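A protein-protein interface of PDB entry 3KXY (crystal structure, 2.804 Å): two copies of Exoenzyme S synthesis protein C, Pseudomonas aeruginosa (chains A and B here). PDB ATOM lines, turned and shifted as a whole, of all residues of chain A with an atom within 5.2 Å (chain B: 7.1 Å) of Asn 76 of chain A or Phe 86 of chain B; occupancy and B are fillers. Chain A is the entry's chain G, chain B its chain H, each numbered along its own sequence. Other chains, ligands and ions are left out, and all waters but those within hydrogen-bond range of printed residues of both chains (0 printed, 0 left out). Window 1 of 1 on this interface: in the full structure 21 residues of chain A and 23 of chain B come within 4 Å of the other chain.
Asn 76 of chain B touches its own counterpart, Asn 76 of chain A. Asn 76 of chain A touches His 85 of chain B, and with the chains exchanged His 85 of chain A touches Asn 76 of chain B. Asn 76 of chain A touches Phe 86 of chain B, and with the chains exchanged Phe 86 of chain A touches Asn 76 of chain B. Trp 79 of chain A touches His 85 of chain B, but with the chains exchanged His 85 of chain A does not touch Trp 79 of chain B (6.1 Å). 9 positions are printed for both chains.
Gly 87 of chain B touches Ala 73 of chain A (CA to O, 3.5 Å). Phe 88 of chain B touches Ser 74 of chain A (O to CA, 3.9 Å). O of Asn 76 of chain A touches CE1 of His 85 of chain B (3.2 Å). Phe 88 of chain B touches Arg 77 of chain A. Gln 96 of chain B touches Arg 77 of chain A. OH of Tyr 98 of chain B touches CG of Arg 77 of chain A, at 3.2 Å. Trp 79 of chain A touches Tyr 98 of chain B. His 85 of chain A touches Asn 76 of chain B (NE2 to O, 3.9 Å). Asn 76 of chain B touches Phe 86 of chain A (ND2 to O, 3.5 Å).
NE2 of His 78 of chain A lies within hydrogen-bond range of NE of Arg 77 of chain A (3.3 Å). OD1 of Asn 76 of chain B lies within hydrogen-bond range of N of Phe 86 of chain B (2.7 Å). O of Leu 72 of chain A sits close to OD1 of Asn 76 of chain A, at 3.4 Å. OD1 of Asn 76 of chain A lies within hydrogen-bond range of N of Phe 86 of chain A, 2.9 Å away. The side-chain amide oxygen (OE1) of Gln 96 of chain B is in hydrogen-bond range of the side-chain hydroxyl (OH) of Tyr 98 of chain B, at 3.0 Å. OD1 of Asn 76 of chain B sits close to O of Leu 72 of chain B, 3.2 Å away.
O of Phe 86 of chain B lies within hydrogen-bond range of ND2 of Asn 76 of chain A, at 3.2 Å. NE2 of His 85 of chain B lies close to NE1 of Trp 79 of chain A (3.3 Å). The side-chain amide nitrogen (ND2) of Asn 76 of chain B sits close to the side-chain amide nitrogen (ND2) of Asn 76 of chain A. The backbone carbonyl oxygen (O) of Ala 73 of chain A is in hydrogen-bond range of the backbone NH (N) of Phe 88 of chain B, 3.5 Å away.
Of chain B, only Asn 76, His 85 and Phe 86 come within 4 Å of Asn 76 of chain A. Printed residues of chain B within 4 Å of Arg 77 of chain A: Phe 88 (3.2 Å), Gln 96 (3.95 Å) and Tyr 98 (3.2 Å). Of the printed residues of chain B, Trp 79 of chain A touches His 85 and Tyr 98. Of the printed residues of chain B, His 85 of chain A touches Asn 76. Trp 79 of chain B touches none of the printed residues of chain A. Phe 86 of chain B touches one residue of chain A. Of the printed residues of chain A, Gly 87 of chain B touches Ala 73. Of the printed residues of chain A, Gln 96 of chain B touches Arg 77. The nearest printed residue of chain B that does not touch Asn 76 of chain A is Tyr 98 of chain B (4.05 Å). The nearest printed residue of chain A that does not touch Gly 87 of chain B is Asn 76 of chain A (4.1 Å).
Of the 11 printed residues of chain A, 7 touch a printed residue of chain B. Hydrophobic or aromatic side chains of chain A that line the printed part of chain B: Trp 79 and His 85. Of the 21 printed residues of chain B, 7 touch a printed residue of chain A. Hydrophobic or aromatic side chains of chain B within 4 Å of the printed part of chain A: His 85 and Tyr 98. Along chain B the printed residues that touch a printed residue of chain A span positions 76 to 98. Among the printed residues, 13 pairs touch across the chains.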
ATOM      1  N   LEU A  72       2.894 -13.986 -19.534  1.00  0.00           N
ATOM      2  CA  LEU A  72       3.613 -12.755 -19.841  1.00  0.00           C
ATOM      3  C   LEU A  72       4.341 -12.254 -18.599  1.00  0.00           C
ATOM      4  O   LEU A  72       5.446 -11.719 -18.688  1.00  0.00           O
ATOM      5  CB  LEU A  72       2.655 -11.680 -20.357  1.00  0.00           C
ATOM      6  CG  LEU A  72       1.949 -11.964 -21.684  1.00  0.00           C
ATOM      7  CD1 LEU A  72       1.011 -10.822 -22.044  1.00  0.00           C
ATOM      8  CD2 LEU A  72       2.961 -12.198 -22.794  1.00  0.00           C
ATOM      9  N   ALA A  73       3.713 -12.433 -17.442  1.00  0.00           N
ATOM     10  CA  ALA A  73       4.327 -12.056 -16.176  1.00  0.00           C
ATOM     11  C   ALA A  73       5.527 -12.948 -15.883  1.00  0.00           C
ATOM     12  O   ALA A  73       6.569 -12.473 -15.433  1.00  0.00           O
ATOM     13  CB  ALA A  73       3.311 -12.134 -15.047  1.00  0.00           C
ATOM     14  N   SER A  74       5.377 -14.243 -16.145  1.00  0.00           N
ATOM     15  CA  SER A  74       6.470 -15.191 -15.954  1.00  0.00           C
ATOM     16  C   SER A  74       7.663 -14.811 -16.821  1.00  0.00           C
ATOM     17  O   SER A  74       8.806 -15.120 -16.489  1.00  0.00           O
ATOM     18  CB  SER A  74       6.017 -16.614 -16.279  1.00  0.00           C
ATOM     19  OG  SER A  74       4.998 -17.040 -15.392  1.00  0.00           O
ATOM     20  N   PHE A  75       7.387 -14.142 -17.936  1.00  0.00           N
ATOM     21  CA  PHE A  75       8.440 -13.674 -18.828  1.00  0.00           C
ATOM     22  C   PHE A  75       9.217 -12.532 -18.183  1.00  0.00           C
ATOM     23  O   PHE A  75      10.449 -12.530 -18.182  1.00  0.00           O
ATOM     24  CB  PHE A  75       7.852 -13.218 -20.163  1.00  0.00           C
ATOM     25  CG  PHE A  75       8.868 -12.639 -21.107  1.00  0.00           C
ATOM     26  CD1 PHE A  75       9.505 -13.441 -22.039  1.00  0.00           C
ATOM     27  CD2 PHE A  75       9.189 -11.292 -21.061  1.00  0.00           C
ATOM     28  CE1 PHE A  75      10.440 -12.911 -22.907  1.00  0.00           C
ATOM     29  CE2 PHE A  75      10.123 -10.758 -21.925  1.00  0.00           C
ATOM     30  CZ  PHE A  75      10.750 -11.567 -22.849  1.00  0.00           C
ATOM     31  N   ASN A  76       8.487 -11.565 -17.636  1.00  0.00           N
ATOM     32  CA  ASN A  76       9.095 -10.402 -16.997  1.00  0.00           C
ATOM     33  C   ASN A  76      10.083 -10.778 -15.898  1.00  0.00           C
ATOM     34  O   ASN A  76      10.977 -10.000 -15.566  1.00  0.00           O
ATOM     35  CB  ASN A  76       8.016  -9.473 -16.439  1.00  0.00           C
ATOM     36  CG  ASN A  76       7.135  -8.885 -17.523  1.00  0.00           C
ATOM     37  OD1 ASN A  76       7.464  -8.950 -18.706  1.00  0.00           O
ATOM     38  ND2 ASN A  76       6.009  -8.306 -17.123  1.00  0.00           N
ATOM     39  N   ARG A  77       9.914 -11.969 -15.334  1.00  0.00           N
ATOM     40  CA  ARG A  77      10.823 -12.463 -14.308  1.00  0.00           C
ATOM     41  C   ARG A  77      12.232 -12.628 -14.867  1.00  0.00           C
ATOM     42  O   ARG A  77      13.218 -12.462 -14.146  1.00  0.00           O
ATOM     43  CB  ARG A  77      10.319 -13.788 -13.733  1.00  0.00           C
ATOM     44  CG  ARG A  77      11.350 -14.534 -12.898  1.00  0.00           C
ATOM     45  CD  ARG A  77      10.778 -15.822 -12.328  1.00  0.00           C
ATOM     46  NE  ARG A  77      11.830 -16.725 -11.868  1.00  0.00           N
ATOM     47  CZ  ARG A  77      12.402 -16.660 -10.671  1.00  0.00           C
ATOM     48  NH1 ARG A  77      12.030 -15.728  -9.804  1.00  0.00           N
ATOM     49  NH2 ARG A  77      13.351 -17.526 -10.341  1.00  0.00           N
ATOM     50  N   HIS A  78      12.321 -12.950 -16.153  1.00  0.00           N
ATOM     51  CA  HIS A  78      13.610 -13.110 -16.818  1.00  0.00           C
ATOM     52  C   HIS A  78      13.764 -12.121 -17.969  1.00  0.00           C
ATOM     53  O   HIS A  78      14.349 -12.441 -19.004  1.00  0.00           O
ATOM     54  CB  HIS A  78      13.778 -14.542 -17.332  1.00  0.00           C
ATOM     55  CG  HIS A  78      13.648 -15.583 -16.267  1.00  0.00           C
ATOM     56  ND1 HIS A  78      14.664 -15.871 -15.380  1.00  0.00           N
ATOM     57  CD2 HIS A  78      12.624 -16.408 -15.946  1.00  0.00           C
ATOM     58  CE1 HIS A  78      14.269 -16.826 -14.557  1.00  0.00           C
ATOM     59  NE2 HIS A  78      13.035 -17.170 -14.879  1.00  0.00           N
ATOM     60  N   TRP A  79      13.236 -10.916 -17.780  1.00  0.00           N
ATOM     61  CA  TRP A  79      13.297  -9.886 -18.807  1.00  0.00           C
ATOM     62  C   TRP A  79      14.743  -9.509 -19.110  1.00  0.00           C
ATOM     63  O   TRP A  79      15.054  -9.037 -20.202  1.00  0.00           O
ATOM     64  CB  TRP A  79      12.521  -8.645 -18.361  1.00  0.00           C
ATOM     65  CG  TRP A  79      13.346  -7.670 -17.574  1.00  0.00           C
ATOM     66  CD1 TRP A  79      13.770  -6.438 -17.983  1.00  0.00           C
ATOM     67  CD2 TRP A  79      13.859  -7.850 -16.249  1.00  0.00           C
ATOM     68  NE1 TRP A  79      14.508  -5.837 -16.991  1.00  0.00           N
ATOM     69  CE2 TRP A  79      14.579  -6.685 -15.917  1.00  0.00           C
ATOM     70  CE3 TRP A  79      13.779  -8.882 -15.309  1.00  0.00           C
ATOM     71  CZ2 TRP A  79      15.211  -6.523 -14.686  1.00  0.00           C
ATOM     72  CZ3 TRP A  79      14.407  -8.720 -14.089  1.00  0.00           C
ATOM     73  CH2 TRP A  79      15.114  -7.549 -13.789  1.00  0.00           C
ATOM     74  N   LEU A  84      13.828  -6.788 -22.411  1.00  0.00           N
ATOM     75  CA  LEU A  84      12.483  -6.462 -22.866  1.00  0.00           C
ATOM     76  C   LEU A  84      11.455  -7.022 -21.893  1.00  0.00           C
ATOM     77  O   LEU A  84      11.581  -8.156 -21.434  1.00  0.00           O
ATOM     78  CB  LEU A  84      12.237  -7.053 -24.257  1.00  0.00           C
ATOM     79  CG  LEU A  84      13.172  -6.629 -25.392  1.00  0.00           C
ATOM     80  CD1 LEU A  84      13.115  -7.627 -26.538  1.00  0.00           C
ATOM     81  CD2 LEU A  84      12.836  -5.228 -25.874  1.00  0.00           C
ATOM     82  N   HIS A  85      10.435  -6.229 -21.578  1.00  0.00           N
ATOM     83  CA  HIS A  85       9.357  -6.703 -20.719  1.00  0.00           C
ATOM     84  C   HIS A  85       7.984  -6.347 -21.286  1.00  0.00           C
ATOM     85  O   HIS A  85       7.847  -5.400 -22.059  1.00  0.00           O
ATOM     86  CB  HIS A  85       9.515  -6.177 -19.288  1.00  0.00           C
ATOM     87  CG  HIS A  85       9.350  -4.695 -19.162  1.00  0.00           C
ATOM     88  ND1 HIS A  85      10.402  -3.815 -19.288  1.00  0.00           N
ATOM     89  CD2 HIS A  85       8.255  -3.939 -18.906  1.00  0.00           C
ATOM     90  CE1 HIS A  85       9.964  -2.579 -19.123  1.00  0.00           C
ATOM     91  NE2 HIS A  85       8.664  -2.627 -18.890  1.00  0.00           N
ATOM     92  N   PHE A  86       6.973  -7.120 -20.898  1.00  0.00           N
ATOM     93  CA  PHE A  86       5.620  -6.933 -21.408  1.00  0.00           C
ATOM     94  C   PHE A  86       4.811  -5.936 -20.588  1.00  0.00           C
ATOM     95  O   PHE A  86       5.023  -5.782 -19.386  1.00  0.00           O
ATOM     96  CB  PHE A  86       4.875  -8.270 -21.461  1.00  0.00           C
ATOM     97  CG  PHE A  86       5.272  -9.141 -22.615  1.00  0.00           C
ATOM     98  CD1 PHE A  86       4.659  -8.999 -23.848  1.00  0.00           C
ATOM     99  CD2 PHE A  86       6.254 -10.106 -22.467  1.00  0.00           C
ATOM    100  CE1 PHE A  86       5.020  -9.802 -24.914  1.00  0.00           C
ATOM    101  CE2 PHE A  86       6.619 -10.912 -23.528  1.00  0.00           C
ATOM    102  CZ  PHE A  86       6.002 -10.759 -24.754  1.00  0.00           C
ATOM    103  N   VAL B  58       6.508  -9.309  -3.248  1.00  0.00           N
ATOM    104  CA  VAL B  58       5.436  -8.384  -2.905  1.00  0.00           C
ATOM    105  C   VAL B  58       4.319  -9.102  -2.153  1.00  0.00           C
ATOM    106  O   VAL B  58       4.241  -9.030  -0.927  1.00  0.00           O
ATOM    107  CB  VAL B  58       4.862  -7.700  -4.156  1.00  0.00           C
ATOM    108  CG1 VAL B  58       4.000  -6.509  -3.759  1.00  0.00           C
ATOM    109  CG2 VAL B  58       5.991  -7.264  -5.076  1.00  0.00           C
ATOM    110  N   GLN B  71      -4.016  -6.550 -14.534  1.00  0.00           N
ATOM    111  CA  GLN B  71      -3.603  -5.308 -13.894  1.00  0.00           C
ATOM    112  C   GLN B  71      -2.085  -5.150 -13.873  1.00  0.00           C
ATOM    113  O   GLN B  71      -1.562  -4.096 -14.233  1.00  0.00           O
ATOM    114  CB  GLN B  71      -4.165  -5.227 -12.473  1.00  0.00           C
ATOM    115  CG  GLN B  71      -5.685  -5.232 -12.406  1.00  0.00           C
ATOM    116  CD  GLN B  71      -6.206  -5.197 -10.982  1.00  0.00           C
ATOM    117  OE1 GLN B  71      -5.433  -5.243 -10.025  1.00  0.00           O
ATOM    118  NE2 GLN B  71      -7.523  -5.116 -10.837  1.00  0.00           N
ATOM    119  N   LEU B  72      -1.384  -6.198 -13.452  1.00  0.00           N
ATOM    120  CA  LEU B  72       0.075  -6.166 -13.393  1.00  0.00           C
ATOM    121  C   LEU B  72       0.676  -5.726 -14.723  1.00  0.00           C
ATOM    122  O   LEU B  72       1.520  -4.830 -14.766  1.00  0.00           O
ATOM    123  CB  LEU B  72       0.636  -7.531 -12.989  1.00  0.00           C
ATOM    124  CG  LEU B  72       0.407  -7.963 -11.540  1.00  0.00           C
ATOM    125  CD1 LEU B  72       1.040  -9.321 -11.282  1.00  0.00           C
ATOM    126  CD2 LEU B  72       0.955  -6.922 -10.575  1.00  0.00           C
ATOM    127  N   ALA B  73       0.238  -6.360 -15.804  1.00  0.00           N
ATOM    128  CA  ALA B  73       0.705  -6.004 -17.138  1.00  0.00           C
ATOM    129  C   ALA B  73       0.478  -4.520 -17.407  1.00  0.00           C
ATOM    130  O   ALA B  73       1.331  -3.845 -17.983  1.00  0.00           O
ATOM    131  CB  ALA B  73       0.004  -6.851 -18.189  1.00  0.00           C
ATOM    132  N   SER B  74      -0.676  -4.017 -16.979  1.00  0.00           N
ATOM    133  CA  SER B  74      -1.021  -2.615 -17.175  1.00  0.00           C
ATOM    134  C   SER B  74      -0.131  -1.697 -16.340  1.00  0.00           C
ATOM    135  O   SER B  74       0.286  -0.636 -16.803  1.00  0.00           O
ATOM    136  CB  SER B  74      -2.494  -2.370 -16.842  1.00  0.00           C
ATOM    137  OG  SER B  74      -2.866  -1.036 -17.141  1.00  0.00           O
ATOM    138  N   PHE B  75       0.156  -2.112 -15.110  1.00  0.00           N
ATOM    139  CA  PHE B  75       1.025  -1.339 -14.230  1.00  0.00           C
ATOM    140  C   PHE B  75       2.414  -1.175 -14.838  1.00  0.00           C
ATOM    141  O   PHE B  75       3.022  -0.109 -14.741  1.00  0.00           O
ATOM    142  CB  PHE B  75       1.140  -2.003 -12.855  1.00  0.00           C
ATOM    143  CG  PHE B  75      -0.152  -2.046 -12.091  1.00  0.00           C
ATOM    144  CD1 PHE B  75      -0.870  -0.886 -11.851  1.00  0.00           C
ATOM    145  CD2 PHE B  75      -0.637  -3.243 -11.594  1.00  0.00           C
ATOM    146  CE1 PHE B  75      -2.056  -0.922 -11.142  1.00  0.00           C
ATOM    147  CE2 PHE B  75      -1.823  -3.286 -10.884  1.00  0.00           C
ATOM    148  CZ  PHE B  75      -2.533  -2.125 -10.658  1.00  0.00           C
ATOM    149  N   ASN B  76       2.908  -2.239 -15.464  1.00  0.00           N
ATOM    150  CA  ASN B  76       4.241  -2.235 -16.057  1.00  0.00           C
ATOM    151  C   ASN B  76       4.401  -1.195 -17.158  1.00  0.00           C
ATOM    152  O   ASN B  76       5.521  -0.826 -17.514  1.00  0.00           O
ATOM    153  CB  ASN B  76       4.595  -3.623 -16.592  1.00  0.00           C
ATOM    154  CG  ASN B  76       4.783  -4.640 -15.487  1.00  0.00           C
ATOM    155  OD1 ASN B  76       4.668  -4.316 -14.306  1.00  0.00           O
ATOM    156  ND2 ASN B  76       5.077  -5.878 -15.865  1.00  0.00           N
ATOM    157  N   TRP B  79       4.928   2.038 -14.798  1.00  0.00           N
ATOM    158  CA  TRP B  79       6.095   1.829 -13.948  1.00  0.00           C
ATOM    159  C   TRP B  79       7.354   1.669 -14.790  1.00  0.00           C
ATOM    160  O   TRP B  79       8.451   1.475 -14.265  1.00  0.00           O
ATOM    161  CB  TRP B  79       5.895   0.618 -13.036  1.00  0.00           C
ATOM    162  CG  TRP B  79       5.623   0.996 -11.615  1.00  0.00           C
ATOM    163  CD1 TRP B  79       6.388   0.697 -10.526  1.00  0.00           C
ATOM    164  CD2 TRP B  79       4.517   1.765 -11.130  1.00  0.00           C
ATOM    165  NE1 TRP B  79       5.821   1.224  -9.390  1.00  0.00           N
ATOM    166  CE2 TRP B  79       4.672   1.885  -9.735  1.00  0.00           C
ATOM    167  CE3 TRP B  79       3.408   2.361 -11.740  1.00  0.00           C
ATOM    168  CZ2 TRP B  79       3.761   2.577  -8.940  1.00  0.00           C
ATOM    169  CZ3 TRP B  79       2.504   3.045 -10.949  1.00  0.00           C
ATOM    170  CH2 TRP B  79       2.686   3.148  -9.564  1.00  0.00           C
ATOM    171  N   LEU B  84      11.002  -0.010 -13.172  1.00  0.00           N
ATOM    172  CA  LEU B  84      10.554  -1.157 -12.393  1.00  0.00           C
ATOM    173  C   LEU B  84       9.428  -1.860 -13.138  1.00  0.00           C
ATOM    174  O   LEU B  84       8.820  -1.285 -14.041  1.00  0.00           O
ATOM    175  CB  LEU B  84      10.062  -0.716 -11.013  1.00  0.00           C
ATOM    176  CG  LEU B  84      11.092  -0.130 -10.047  1.00  0.00           C
ATOM    177  CD1 LEU B  84      10.410   0.404  -8.796  1.00  0.00           C
ATOM    178  CD2 LEU B  84      12.141  -1.170  -9.690  1.00  0.00           C
ATOM    179  N   HIS B  85       9.151  -3.104 -12.762  1.00  0.00           N
ATOM    180  CA  HIS B  85       8.069  -3.859 -13.384  1.00  0.00           C
ATOM    181  C   HIS B  85       7.716  -5.104 -12.578  1.00  0.00           C
ATOM    182  O   HIS B  85       8.555  -5.654 -11.864  1.00  0.00           O
ATOM    183  CB  HIS B  85       8.431  -4.241 -14.821  1.00  0.00           C
ATOM    184  CG  HIS B  85       9.691  -5.041 -14.934  1.00  0.00           C
ATOM    185  ND1 HIS B  85       9.700  -6.420 -14.937  1.00  0.00           N
ATOM    186  CD2 HIS B  85      10.984  -4.657 -15.045  1.00  0.00           C
ATOM    187  CE1 HIS B  85      10.944  -6.849 -15.048  1.00  0.00           C
ATOM    188  NE2 HIS B  85      11.743  -5.799 -15.113  1.00  0.00           N
ATOM    189  N   PHE B  86       6.468  -5.541 -12.698  1.00  0.00           N
ATOM    190  CA  PHE B  86       5.988  -6.712 -11.977  1.00  0.00           C
ATOM    191  C   PHE B  86       6.241  -7.998 -12.759  1.00  0.00           C
ATOM    192  O   PHE B  86       6.040  -8.051 -13.971  1.00  0.00           O
ATOM    193  CB  PHE B  86       4.496  -6.580 -11.668  1.00  0.00           C
ATOM    194  CG  PHE B  86       4.171  -5.481 -10.697  1.00  0.00           C
ATOM    195  CD1 PHE B  86       4.144  -5.728  -9.334  1.00  0.00           C
ATOM    196  CD2 PHE B  86       3.888  -4.201 -11.146  1.00  0.00           C
ATOM    197  CE1 PHE B  86       3.843  -4.718  -8.437  1.00  0.00           C
ATOM    198  CE2 PHE B  86       3.586  -3.188 -10.253  1.00  0.00           C
ATOM    199  CZ  PHE B  86       3.564  -3.448  -8.898  1.00  0.00           C
ATOM    200  N   GLY B  87       6.681  -9.031 -12.050  1.00  0.00           N
ATOM    201  CA  GLY B  87       6.874 -10.344 -12.636  1.00  0.00           C
ATOM    202  C   GLY B  87       6.316 -11.409 -11.713  1.00  0.00           C
ATOM    203  O   GLY B  87       5.568 -11.100 -10.787  1.00  0.00           O
ATOM    204  N   PHE B  88       6.679 -12.663 -11.956  1.00  0.00           N
ATOM    205  CA  PHE B  88       6.191 -13.756 -11.126  1.00  0.00           C
ATOM    206  C   PHE B  88       7.082 -14.996 -11.183  1.00  0.00           C
ATOM    207  O   PHE B  88       7.574 -15.372 -12.248  1.00  0.00           O
ATOM    208  CB  PHE B  88       4.755 -14.122 -11.509  1.00  0.00           C
ATOM    209  CG  PHE B  88       4.233 -15.336 -10.799  1.00  0.00           C
ATOM    210  CD1 PHE B  88       3.852 -15.266  -9.469  1.00  0.00           C
ATOM    211  CD2 PHE B  88       4.124 -16.548 -11.459  1.00  0.00           C
ATOM    212  CE1 PHE B  88       3.374 -16.381  -8.812  1.00  0.00           C
ATOM    213  CE2 PHE B  88       3.645 -17.667 -10.807  1.00  0.00           C
ATOM    214  CZ  PHE B  88       3.272 -17.585  -9.481  1.00  0.00           C
ATOM    215  N   VAL B  95       4.090 -12.833  -6.577  1.00  0.00           N
ATOM    216  CA  VAL B  95       4.398 -11.730  -7.481  1.00  0.00           C
ATOM    217  C   VAL B  95       5.581 -10.918  -6.959  1.00  0.00           C
ATOM    218  O   VAL B  95       5.707 -10.700  -5.755  1.00  0.00           O
ATOM    219  CB  VAL B  95       3.182 -10.802  -7.660  1.00  0.00           C
ATOM    220  CG1 VAL B  95       3.524  -9.645  -8.585  1.00  0.00           C
ATOM    221  CG2 VAL B  95       1.994 -11.587  -8.197  1.00  0.00           C
ATOM    222  N   GLN B  96       6.445 -10.473  -7.866  1.00  0.00           N
ATOM    223  CA  GLN B  96       7.658  -9.761  -7.472  1.00  0.00           C
ATOM    224  C   GLN B  96       7.893  -8.480  -8.271  1.00  0.00           C
ATOM    225  O   GLN B  96       7.392  -8.325  -9.383  1.00  0.00           O
ATOM    226  CB  GLN B  96       8.877 -10.677  -7.603  1.00  0.00           C
ATOM    227  CG  GLN B  96       8.824 -11.920  -6.727  1.00  0.00           C
ATOM    228  CD  GLN B  96      10.032 -12.819  -6.917  1.00  0.00           C
ATOM    229  OE1 GLN B  96      10.900 -12.548  -7.748  1.00  0.00           O
ATOM    230  NE2 GLN B  96      10.094 -13.899  -6.145  1.00  0.00           N
ATOM    231  N   LEU B  97       8.659  -7.564  -7.684  1.00  0.00           N
ATOM    232  CA  LEU B  97       9.126  -6.370  -8.381  1.00  0.00           C
ATOM    233  C   LEU B  97      10.601  -6.533  -8.730  1.00  0.00           C
ATOM    234  O   LEU B  97      11.410  -6.898  -7.877  1.00  0.00           O
ATOM    235  CB  LEU B  97       8.931  -5.124  -7.516  1.00  0.00           C
ATOM    236  CG  LEU B  97       7.537  -4.497  -7.503  1.00  0.00           C
ATOM    237  CD1 LEU B  97       7.463  -3.379  -6.477  1.00  0.00           C
ATOM    238  CD2 LEU B  97       7.177  -3.980  -8.886  1.00  0.00           C
ATOM    239  N   TYR B  98      10.950  -6.262  -9.983  1.00  0.00           N
ATOM    240  CA  TYR B  98      12.314  -6.484 -10.450  1.00  0.00           C
ATOM    241  C   TYR B  98      13.065  -5.193 -10.758  1.00  0.00           C
ATOM    242  O   TYR B  98      12.464  -4.165 -11.070  1.00  0.00           O
ATOM    243  CB  TYR B  98      12.318  -7.397 -11.677  1.00  0.00           C
ATOM    244  CG  TYR B  98      11.748  -8.771 -11.411  1.00  0.00           C
ATOM    245  CD1 TYR B  98      12.543  -9.785 -10.898  1.00  0.00           C
ATOM    246  CD2 TYR B  98      10.414  -9.052 -11.673  1.00  0.00           C
ATOM    247  CE1 TYR B  98      12.026 -11.043 -10.653  1.00  0.00           C
ATOM    248  CE2 TYR B  98       9.889 -10.306 -11.430  1.00  0.00           C
ATOM    249  CZ  TYR B  98      10.699 -11.297 -10.921  1.00  0.00           C
ATOM    250  OH  TYR B  98      10.177 -12.548 -10.679  1.00  0.00           O
ATOM    251  N   HIS B 121       8.712   1.238  -3.174  1.00  0.00           N
ATOM    252  CA  HIS B 121       7.695   0.735  -4.092  1.00  0.00           C
ATOM    253  C   HIS B 121       7.156  -0.628  -3.660  1.00  0.00           C
ATOM    254  O   HIS B 121       5.975  -0.921  -3.843  1.00  0.00           O
ATOM    255  CB  HIS B 121       8.247   0.657  -5.516  1.00  0.00           C
ATOM    256  CG  HIS B 121       8.314   1.979  -6.216  1.00  0.00           C
ATOM    257  ND1 HIS B 121       7.360   2.386  -7.125  1.00  0.00           N
ATOM    258  CD2 HIS B 121       9.217   2.985  -6.143  1.00  0.00           C
ATOM    259  CE1 HIS B 121       7.675   3.586  -7.583  1.00  0.00           C
ATOM    260  NE2 HIS B 121       8.796   3.972  -7.003  1.00  0.00           N
ATOM    261  N   PHE B 124       4.821   0.070  -0.762  1.00  0.00           N
ATOM    262  CA  PHE B 124       3.679   0.778  -1.332  1.00  0.00           C
ATOM    263  C   PHE B 124       2.658  -0.170  -1.949  1.00  0.00           C
ATOM    264  O   PHE B 124       1.452   0.017  -1.791  1.00  0.00           O
ATOM    265  CB  PHE B 124       4.156   1.788  -2.381  1.00  0.00           C
ATOM    266  CG  PHE B 124       3.070   2.272  -3.305  1.00  0.00           C
ATOM    267  CD1 PHE B 124       2.308   3.382  -2.982  1.00  0.00           C
ATOM    268  CD2 PHE B 124       2.823   1.623  -4.504  1.00  0.00           C
ATOM    269  CE1 PHE B 124       1.314   3.829  -3.834  1.00  0.00           C
ATOM    270  CE2 PHE B 124       1.832   2.064  -5.358  1.00  0.00           C
ATOM    271  CZ  PHE B 124       1.078   3.170  -5.024  1.00  0.00           C
ATOM    272  N   TRP B 125       3.143  -1.188  -2.650  1.00  0.00           N
ATOM    273  CA  TRP B 125       2.260  -2.096  -3.372  1.00  0.00           C
ATOM    274  C   TRP B 125       1.635  -3.174  -2.486  1.00  0.00           C
ATOM    275  O   TRP B 125       0.503  -3.591  -2.718  1.00  0.00           O
ATOM    276  CB  TRP B 125       2.992  -2.732  -4.553  1.00  0.00           C
ATOM    277  CG  TRP B 125       3.104  -1.825  -5.743  1.00  0.00           C
ATOM    278  CD1 TRP B 125       4.234  -1.224  -6.218  1.00  0.00           C
ATOM    279  CD2 TRP B 125       2.037  -1.411  -6.606  1.00  0.00           C
ATOM    280  NE1 TRP B 125       3.937  -0.466  -7.327  1.00  0.00           N
ATOM    281  CE2 TRP B 125       2.594  -0.563  -7.585  1.00  0.00           C
ATOM    282  CE3 TRP B 125       0.665  -1.674  -6.648  1.00  0.00           C
ATOM    283  CZ2 TRP B 125       1.827   0.020  -8.593  1.00  0.00           C
ATOM    284  CZ3 TRP B 125      -0.093  -1.096  -7.648  1.00  0.00           C
ATOM    285  CH2 TRP B 125       0.488  -0.258  -8.606  1.00  0.00           C
ATOM    286  N   LEU B 129      -2.144  -3.977  -3.160  1.00  0.00           N
ATOM    287  CA  LEU B 129      -2.467  -5.155  -3.962  1.00  0.00           C
ATOM    288  C   LEU B 129      -3.780  -5.834  -3.547  1.00  0.00           C
ATOM    289  O   LEU B 129      -4.644  -6.080  -4.391  1.00  0.00           O
ATOM    290  CB  LEU B 129      -1.297  -6.149  -3.982  1.00  0.00           C
ATOM    291  CG  LEU B 129      -0.381  -6.085  -5.211  1.00  0.00           C
ATOM    292  CD1 LEU B 129      -0.036  -4.649  -5.575  1.00  0.00           C
ATOM    293  CD2 LEU B 129       0.884  -6.918  -5.014  1.00  0.00           C
